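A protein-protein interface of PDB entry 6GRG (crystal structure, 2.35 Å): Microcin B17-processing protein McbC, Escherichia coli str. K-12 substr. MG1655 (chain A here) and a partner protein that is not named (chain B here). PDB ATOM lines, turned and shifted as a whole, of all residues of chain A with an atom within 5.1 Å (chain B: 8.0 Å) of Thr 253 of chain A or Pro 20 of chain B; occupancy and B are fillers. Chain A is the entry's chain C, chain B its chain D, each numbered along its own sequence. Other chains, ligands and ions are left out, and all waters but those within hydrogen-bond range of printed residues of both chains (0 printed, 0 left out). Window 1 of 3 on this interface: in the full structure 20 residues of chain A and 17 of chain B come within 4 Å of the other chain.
N of Asp 250 of chain A sits at hydrogen-bond distance from O of Leu 22 of chain B (2.9 Å). OG1 of Thr 12 of chain A sits at hydrogen-bond distance from N of Met 1 of chain B. The side-chain carboxylate (OD2) of Asp 250 of chain A lies within salt-bridge range of the side-chain amino group (NZ) of Lys 21 of chain B, 3.9 Å away. The side-chain hydroxyl of Thr 253 of chain A sits at hydrogen-bond distance from the backbone NH of Lys 21 of chain B (3.1 Å). The backbone NH of Met 1 of chain B sits at hydrogen-bond distance from the side-chain carboxylate of Glu 196 of chain A (2.7 Å). O of Thr 12 of chain A lies within hydrogen-bond range of ND2 of Asn 3 of chain B, at 2.7 Å.
The side-chain hydroxyl (OG1) of Thr 12 of chain A is in hydrogen-bond range of the side-chain carboxylate (OE1) of Glu 196 of chain A, 2.6 Å away. The side-chain hydroxyl (OG1) of Thr 28 of chain B lies within hydrogen-bond range of the side-chain amino group (NZ) of Lys 21 of chain B, at 3.2 Å. The backbone carbonyl oxygen (O) of Arg 252 of chain A sits at hydrogen-bond distance from the side-chain amino group (NZ) of Lys 24 of chain A, at 2.8 Å. The backbone NH of Met 1 of chain B sits at hydrogen-bond distance from the side-chain amide oxygen of Asn 3 of chain B, at 2.9 Å. OD2 of Asp 250 of chain A lies within salt-bridge range of NH2 of Arg 252 of chain A. O of Thr 253 of chain A sits at hydrogen-bond distance from N of Phe 195 of chain A (3.0 Å).
Of the printed residues of chain B, Glu 196 of chain A touches Met 1, Asn 3 and Pro 20. Of the printed residues of chain B, Asp 250 of chain A touches Lys 21 (2.9 Å) and Leu 22 (2.9 Å). Printed residues of chain A within 4 Å of Asn 3 of chain B: Thr 12 (2.7 Å) and Glu 196 (3.9 Å). Pro 20 of chain B touches just these residues of chain A: Leu 8, Thr 12, Glu 196 and Thr 253. The nearest printed residue of chain A that does not touch Pro 20 of chain B is Ile 194 of chain A (5.3 Å).
Of the 13 printed residues of chain B, 6 touch a printed residue of chain A. Hydrophobic or aromatic side chains of chain B within 4 Å of the printed part of chain A: Met 1, Ala 17, Pro 20 and Leu 22. Of the 13 printed residues of chain A, 8 touch a printed residue of chain B. Among the printed residues, 16 pairs touch across the chains.
Leu 8 of chain A touches Pro 20 of chain B. CB of Ala 17 of chain B touches CG2 of Thr 12 of chain A, at 3.7 Å. Pro 20 of chain B touches Thr 12 of chain A. CD1 of Ile 194 of chain A touches CD2 of Leu 22 of chain B, 3.5 Å away. Asn 3 of chain B touches Glu 196 of chain A (OD1 to OE1, 3.9 Å). OE2 of Glu 196 of chain A touches CG of Pro 20 of chain B, 3.4 Å away. SD of Met 1 of chain B touches CB of Arg 252 of chain A, 3.7 Å away. Thr 253 of chain A touches Met 1 of chain B. CA of Pro 20 of chain B touches OG1 of Thr 253 of chain A, at 3.3 Å. CG1 of Val 254 of chain A touches O of Leu 22 of chain B, at 3.8 Å.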
ATOM      1  N   LEU A   8      36.191  18.291 -26.096  1.00  0.00           N
ATOM      2  CA  LEU A   8      35.586  17.613 -24.960  1.00  0.00           C
ATOM      3  C   LEU A   8      36.447  16.430 -24.483  1.00  0.00           C
ATOM      4  O   LEU A   8      36.247  15.947 -23.379  1.00  0.00           O
ATOM      5  CB  LEU A   8      34.170  17.190 -25.354  1.00  0.00           C
ATOM      6  CG  LEU A   8      33.220  18.384 -25.423  1.00  0.00           C
ATOM      7  CD1 LEU A   8      31.821  17.975 -25.861  1.00  0.00           C
ATOM      8  CD2 LEU A   8      33.183  19.101 -24.070  1.00  0.00           C
ATOM      9  N   THR A  12      36.832  15.182 -20.541  1.00  0.00           N
ATOM     10  CA  THR A  12      36.422  13.882 -20.023  1.00  0.00           C
ATOM     11  C   THR A  12      37.540  13.242 -19.190  1.00  0.00           C
ATOM     12  O   THR A  12      37.236  12.372 -18.393  1.00  0.00           O
ATOM     13  CB  THR A  12      35.947  12.921 -21.121  1.00  0.00           C
ATOM     14  OG1 THR A  12      35.193  11.906 -20.454  1.00  0.00           O
ATOM     15  CG2 THR A  12      37.060  12.311 -21.958  1.00  0.00           C
ATOM     16  N   LYS A  24      22.656  12.707 -14.327  1.00  0.00           N
ATOM     17  CA  LYS A  24      21.793  12.433 -15.468  1.00  0.00           C
ATOM     18  C   LYS A  24      20.526  11.708 -15.001  1.00  0.00           C
ATOM     19  O   LYS A  24      19.441  12.033 -15.474  1.00  0.00           O
ATOM     20  CB  LYS A  24      22.484  11.570 -16.522  1.00  0.00           C
ATOM     21  CG  LYS A  24      23.596  12.216 -17.334  1.00  0.00           C
ATOM     22  CD  LYS A  24      24.460  11.120 -17.966  1.00  0.00           C
ATOM     23  CE  LYS A  24      25.191  11.529 -19.225  1.00  0.00           C
ATOM     24  NZ  LYS A  24      25.234  10.420 -20.220  1.00  0.00           N
ATOM     25  N   ILE A 193      22.832  22.126 -21.719  1.00  0.00           N
ATOM     26  CA  ILE A 193      23.916  21.824 -20.820  1.00  0.00           C
ATOM     27  C   ILE A 193      24.754  20.717 -21.462  1.00  0.00           C
ATOM     28  O   ILE A 193      24.192  19.756 -21.924  1.00  0.00           O
ATOM     29  CB  ILE A 193      23.367  21.404 -19.439  1.00  0.00           C
ATOM     30  CG1 ILE A 193      24.500  21.321 -18.422  1.00  0.00           C
ATOM     31  CG2 ILE A 193      22.590  20.093 -19.489  1.00  0.00           C
ATOM     32  CD1 ILE A 193      24.048  21.076 -17.033  1.00  0.00           C
ATOM     33  N   ILE A 194      26.082  20.870 -21.474  1.00  0.00           N
ATOM     34  CA  ILE A 194      27.013  19.763 -21.742  1.00  0.00           C
ATOM     35  C   ILE A 194      27.430  19.164 -20.392  1.00  0.00           C
ATOM     36  O   ILE A 194      28.198  19.769 -19.638  1.00  0.00           O
ATOM     37  CB  ILE A 194      28.228  20.251 -22.543  1.00  0.00           C
ATOM     38  CG1 ILE A 194      27.791  20.952 -23.822  1.00  0.00           C
ATOM     39  CG2 ILE A 194      29.203  19.105 -22.828  1.00  0.00           C
ATOM     40  CD1 ILE A 194      28.960  21.496 -24.612  1.00  0.00           C
ATOM     41  N   PHE A 195      26.892  17.984 -20.075  1.00  0.00           N
ATOM     42  CA  PHE A 195      26.936  17.474 -18.714  1.00  0.00           C
ATOM     43  C   PHE A 195      28.378  17.441 -18.175  1.00  0.00           C
ATOM     44  O   PHE A 195      28.638  17.983 -17.113  1.00  0.00           O
ATOM     45  CB  PHE A 195      26.307  16.081 -18.642  1.00  0.00           C
ATOM     46  CG  PHE A 195      24.820  16.039 -18.860  1.00  0.00           C
ATOM     47  CD1 PHE A 195      23.955  16.612 -17.946  1.00  0.00           C
ATOM     48  CD2 PHE A 195      24.279  15.375 -19.955  1.00  0.00           C
ATOM     49  CE1 PHE A 195      22.579  16.542 -18.130  1.00  0.00           C
ATOM     50  CE2 PHE A 195      22.907  15.323 -20.154  1.00  0.00           C
ATOM     51  CZ  PHE A 195      22.060  15.915 -19.240  1.00  0.00           C
ATOM     52  N   GLU A 196      29.314  16.846 -18.920  1.00  0.00           N
ATOM     53  CA  GLU A 196      30.694  16.643 -18.419  1.00  0.00           C
ATOM     54  C   GLU A 196      31.399  17.993 -18.199  1.00  0.00           C
ATOM     55  O   GLU A 196      32.209  18.159 -17.280  1.00  0.00           O
ATOM     56  CB  GLU A 196      31.452  15.674 -19.336  1.00  0.00           C
ATOM     57  CG  GLU A 196      30.964  14.226 -19.220  1.00  0.00           C
ATOM     58  CD  GLU A 196      31.879  13.148 -19.795  1.00  0.00           C
ATOM     59  OE1 GLU A 196      33.095  13.170 -19.472  1.00  0.00           O
ATOM     60  OE2 GLU A 196      31.374  12.270 -20.580  1.00  0.00           O
ATOM     61  N   ASP A 250      23.443  14.712 -29.342  1.00  0.00           N
ATOM     62  CA  ASP A 250      23.634  13.456 -28.713  1.00  0.00           C
ATOM     63  C   ASP A 250      23.297  13.635 -27.228  1.00  0.00           C
ATOM     64  O   ASP A 250      24.005  14.329 -26.491  1.00  0.00           O
ATOM     65  CB  ASP A 250      25.070  12.998 -28.929  1.00  0.00           C
ATOM     66  CG  ASP A 250      25.370  11.596 -28.428  1.00  0.00           C
ATOM     67  OD1 ASP A 250      24.560  11.050 -27.634  1.00  0.00           O
ATOM     68  OD2 ASP A 250      26.426  11.055 -28.830  1.00  0.00           O
ATOM     69  N   GLN A 251      22.216  12.979 -26.788  1.00  0.00           N
ATOM     70  CA  GLN A 251      21.673  13.152 -25.436  1.00  0.00           C
ATOM     71  C   GLN A 251      22.611  12.585 -24.351  1.00  0.00           C
ATOM     72  O   GLN A 251      22.412  12.877 -23.191  1.00  0.00           O
ATOM     73  CB  GLN A 251      20.292  12.494 -25.330  1.00  0.00           C
ATOM     74  CG  GLN A 251      19.310  12.970 -26.391  1.00  0.00           C
ATOM     75  CD  GLN A 251      17.922  12.433 -26.142  1.00  0.00           C
ATOM     76  OE1 GLN A 251      17.405  12.517 -25.036  1.00  0.00           O
ATOM     77  NE2 GLN A 251      17.310  11.871 -27.171  1.00  0.00           N
ATOM     78  N   ARG A 252      23.579  11.727 -24.699  1.00  0.00           N
ATOM     79  CA  ARG A 252      24.549  11.227 -23.720  1.00  0.00           C
ATOM     80  C   ARG A 252      25.498  12.354 -23.266  1.00  0.00           C
ATOM     81  O   ARG A 252      26.056  12.285 -22.170  1.00  0.00           O
ATOM     82  CB  ARG A 252      25.364  10.074 -24.312  1.00  0.00           C
ATOM     83  CG  ARG A 252      24.576   8.794 -24.545  1.00  0.00           C
ATOM     84  CD  ARG A 252      25.268   7.798 -25.464  1.00  0.00           C
ATOM     85  NE  ARG A 252      25.471   8.345 -26.798  1.00  0.00           N
ATOM     86  CZ  ARG A 252      26.129   7.731 -27.767  1.00  0.00           C
ATOM     87  NH1 ARG A 252      26.651   6.541 -27.546  1.00  0.00           N
ATOM     88  NH2 ARG A 252      26.217   8.278 -28.965  1.00  0.00           N
ATOM     89  N   THR A 253      25.653  13.399 -24.093  1.00  0.00           N
ATOM     90  CA  THR A 253      26.607  14.480 -23.842  1.00  0.00           C
ATOM     91  C   THR A 253      25.923  15.796 -23.465  1.00  0.00           C
ATOM     92  O   THR A 253      26.462  16.575 -22.640  1.00  0.00           O
ATOM     93  CB  THR A 253      27.450  14.692 -25.105  1.00  0.00           C
ATOM     94  OG1 THR A 253      28.281  13.539 -25.202  1.00  0.00           O
ATOM     95  CG2 THR A 253      28.276  15.958 -25.107  1.00  0.00           C
ATOM     96  N   VAL A 254      24.782  16.069 -24.110  1.00  0.00           N
ATOM     97  CA  VAL A 254      24.173  17.391 -24.086  1.00  0.00           C
ATOM     98  C   VAL A 254      22.648  17.250 -24.060  1.00  0.00           C
ATOM     99  O   VAL A 254      22.117  16.374 -24.684  1.00  0.00           O
ATOM    100  CB  VAL A 254      24.630  18.240 -25.290  1.00  0.00           C
ATOM    101  CG1 VAL A 254      24.411  17.545 -26.636  1.00  0.00           C
ATOM    102  CG2 VAL A 254      23.977  19.613 -25.299  1.00  0.00           C
ATOM    103  N   ALA A 255      21.967  18.165 -23.357  1.00  0.00           N
ATOM    104  CA  ALA A 255      20.532  18.137 -23.197  1.00  0.00           C
ATOM    105  C   ALA A 255      19.985  19.560 -23.200  1.00  0.00           C
ATOM    106  O   ALA A 255      20.588  20.455 -22.611  1.00  0.00           O
ATOM    107  CB  ALA A 255      20.154  17.426 -21.916  1.00  0.00           C
ATOM    108  N   MET B   1      32.836   9.972 -20.881  1.00  0.00           N
ATOM    109  CA  MET B   1      32.062   8.791 -20.464  1.00  0.00           C
ATOM    110  C   MET B   1      33.017   7.615 -20.298  1.00  0.00           C
ATOM    111  O   MET B   1      34.201   7.719 -20.714  1.00  0.00           O
ATOM    112  CB  MET B   1      30.969   8.472 -21.486  1.00  0.00           C
ATOM    113  CG  MET B   1      29.660   9.173 -21.126  1.00  0.00           C
ATOM    114  SD  MET B   1      28.543   9.396 -22.518  1.00  0.00           S
ATOM    115  CE  MET B   1      29.436  10.652 -23.447  1.00  0.00           C
ATOM    116  N   ILE B   2      32.488   6.524 -19.710  1.00  0.00           N
ATOM    117  CA  ILE B   2      33.241   5.329 -19.282  1.00  0.00           C
ATOM    118  C   ILE B   2      34.117   5.698 -18.074  1.00  0.00           C
ATOM    119  O   ILE B   2      33.855   5.289 -16.921  1.00  0.00           O
ATOM    120  CB  ILE B   2      34.105   4.738 -20.402  1.00  0.00           C
ATOM    121  CG1 ILE B   2      33.377   4.598 -21.743  1.00  0.00           C
ATOM    122  CG2 ILE B   2      34.700   3.426 -19.939  1.00  0.00           C
ATOM    123  CD1 ILE B   2      32.329   3.550 -21.783  1.00  0.00           C
ATOM    124  N   ASN B   3      35.189   6.444 -18.359  1.00  0.00           N
ATOM    125  CA  ASN B   3      36.053   7.043 -17.371  1.00  0.00           C
ATOM    126  C   ASN B   3      36.484   6.015 -16.307  1.00  0.00           C
ATOM    127  O   ASN B   3      36.327   6.258 -15.127  1.00  0.00           O
ATOM    128  CB  ASN B   3      35.369   8.277 -16.799  1.00  0.00           C
ATOM    129  CG  ASN B   3      35.107   9.316 -17.868  1.00  0.00           C
ATOM    130  OD1 ASN B   3      33.958   9.583 -18.203  1.00  0.00           O
ATOM    131  ND2 ASN B   3      36.154   9.880 -18.445  1.00  0.00           N
ATOM    132  N   ALA B  17      38.539   6.375 -21.643  1.00  0.00           N
ATOM    133  CA  ALA B  17      37.418   7.291 -21.769  1.00  0.00           C
ATOM    134  C   ALA B  17      36.846   7.219 -23.188  1.00  0.00           C
ATOM    135  O   ALA B  17      37.567   6.985 -24.191  1.00  0.00           O
ATOM    136  CB  ALA B  17      37.841   8.697 -21.435  1.00  0.00           C
ATOM    137  N   MET B  18      35.524   7.374 -23.244  1.00  0.00           N
ATOM    138  CA  MET B  18      34.774   7.640 -24.463  1.00  0.00           C
ATOM    139  C   MET B  18      34.468   9.139 -24.485  1.00  0.00           C
ATOM    140  O   MET B  18      33.952   9.669 -23.534  1.00  0.00           O
ATOM    141  CB  MET B  18      33.463   6.848 -24.493  1.00  0.00           C
ATOM    142  CG  MET B  18      32.497   7.314 -25.583  1.00  0.00           C
ATOM    143  SD  MET B  18      31.102   6.173 -25.763  1.00  0.00           S
ATOM    144  CE  MET B  18      29.778   7.059 -24.939  1.00  0.00           C
ATOM    145  N   SER B  19      34.812   9.807 -25.576  1.00  0.00           N
ATOM    146  CA  SER B  19      34.767  11.249 -25.599  1.00  0.00           C
ATOM    147  C   SER B  19      33.325  11.739 -25.776  1.00  0.00           C
ATOM    148  O   SER B  19      32.628  11.306 -26.675  1.00  0.00           O
ATOM    149  CB  SER B  19      35.668  11.789 -26.677  1.00  0.00           C
ATOM    150  OG  SER B  19      35.436  13.182 -26.797  1.00  0.00           O
ATOM    151  N   PRO B  20      32.814  12.671 -24.949  1.00  0.00           N
ATOM    152  CA  PRO B  20      31.541  13.309 -25.253  1.00  0.00           C
ATOM    153  C   PRO B  20      31.648  13.965 -26.631  1.00  0.00           C
ATOM    154  O   PRO B  20      32.758  14.240 -27.062  1.00  0.00           O
ATOM    155  CB  PRO B  20      31.309  14.381 -24.163  1.00  0.00           C
ATOM    156  CG  PRO B  20      32.455  14.233 -23.175  1.00  0.00           C
ATOM    157  CD  PRO B  20      33.398  13.157 -23.692  1.00  0.00           C
ATOM    158  N   LYS B  21      30.489  14.213 -27.250  1.00  0.00           N
ATOM    159  CA  LYS B  21      30.334  15.001 -28.473  1.00  0.00           C
ATOM    160  C   LYS B  21      28.916  15.603 -28.534  1.00  0.00           C
ATOM    161  O   LYS B  21      27.941  14.987 -28.066  1.00  0.00           O
ATOM    162  CB  LYS B  21      30.584  14.089 -29.676  1.00  0.00           C
ATOM    163  CG  LYS B  21      29.838  12.777 -29.585  1.00  0.00           C
ATOM    164  CD  LYS B  21      29.722  12.053 -30.880  1.00  0.00           C
ATOM    165  CE  LYS B  21      28.557  11.095 -30.868  1.00  0.00           C
ATOM    166  NZ  LYS B  21      28.933   9.831 -31.518  1.00  0.00           N
ATOM    167  N   LEU B  22      28.795  16.799 -29.115  1.00  0.00           N
ATOM    168  CA  LEU B  22      27.498  17.454 -29.274  1.00  0.00           C
ATOM    169  C   LEU B  22      26.645  16.748 -30.332  1.00  0.00           C
ATOM    170  O   LEU B  22      25.449  16.633 -30.155  1.00  0.00           O
ATOM    171  CB  LEU B  22      27.705  18.908 -29.683  1.00  0.00           C
ATOM    172  CG  LEU B  22      28.337  19.809 -28.631  1.00  0.00           C
ATOM    173  CD1 LEU B  22      28.176  21.275 -29.026  1.00  0.00           C
ATOM    174  CD2 LEU B  22      27.723  19.552 -27.260  1.00  0.00           C
ATOM    175  N   ASN B  23      27.280  16.330 -31.434  1.00  0.00           N
ATOM    176  CA  ASN B  23      26.640  15.924 -32.692  1.00  0.00           C
ATOM    177  C   ASN B  23      26.449  14.399 -32.716  1.00  0.00           C
ATOM    178  O   ASN B  23      27.430  13.643 -32.630  1.00  0.00           O
ATOM    179  CB  ASN B  23      27.502  16.393 -33.861  1.00  0.00           C
ATOM    180  CG  ASN B  23      26.864  16.110 -35.200  1.00  0.00           C
ATOM    181  OD1 ASN B  23      25.819  15.464 -35.252  1.00  0.00           O
ATOM    182  ND2 ASN B  23      27.470  16.598 -36.270  1.00  0.00           N
ATOM    183  N   PRO B  27      31.089  10.413 -35.444  1.00  0.00           N
ATOM    184  CA  PRO B  27      31.510   9.155 -34.827  1.00  0.00           C
ATOM    185  C   PRO B  27      32.004   9.345 -33.387  1.00  0.00           C
ATOM    186  O   PRO B  27      32.548  10.376 -33.022  1.00  0.00           O
ATOM    187  CB  PRO B  27      32.682   8.713 -35.707  1.00  0.00           C
ATOM    188  CG  PRO B  27      33.271  10.028 -36.182  1.00  0.00           C
ATOM    189  CD  PRO B  27      32.071  10.926 -36.409  1.00  0.00           C
ATOM    190  N   THR B  28      31.811   8.304 -32.595  1.00  0.00           N
ATOM    191  CA  THR B  28      32.401   8.141 -31.309  1.00  0.00           C
ATOM    192  C   THR B  28      33.906   7.885 -31.451  1.00  0.00           C
ATOM    193  O   THR B  28      34.343   7.083 -32.268  1.00  0.00           O
ATOM    194  CB  THR B  28      31.773   6.943 -30.586  1.00  0.00           C
ATOM    195  OG1 THR B  28      30.358   7.079 -30.680  1.00  0.00           O
ATOM    196  CG2 THR B  28      32.183   6.848 -29.133  1.00  0.00           C
ATOM    197  N   PHE B  29      34.671   8.565 -30.595  1.00  0.00           N
ATOM    198  CA  PHE B  29      36.076   8.375 -30.384  1.00  0.00           C
ATOM    199  C   PHE B  29      36.247   7.852 -28.958  1.00  0.00           C
ATOM    200  O   PHE B  29      35.614   8.372 -28.052  1.00  0.00           O
ATOM    201  CB  PHE B  29      36.810   9.701 -30.601  1.00  0.00           C
ATOM    202  CG  PHE B  29      38.296   9.613 -30.404  1.00  0.00           C
ATOM    203  CD1 PHE B  29      39.120   9.178 -31.432  1.00  0.00           C
ATOM    204  CD2 PHE B  29      38.870   9.948 -29.183  1.00  0.00           C
ATOM    205  CE1 PHE B  29      40.490   9.074 -31.236  1.00  0.00           C
ATOM    206  CE2 PHE B  29      40.244   9.851 -28.994  1.00  0.00           C
ATOM    207  CZ  PHE B  29      41.050   9.411 -30.024  1.00  0.00           C
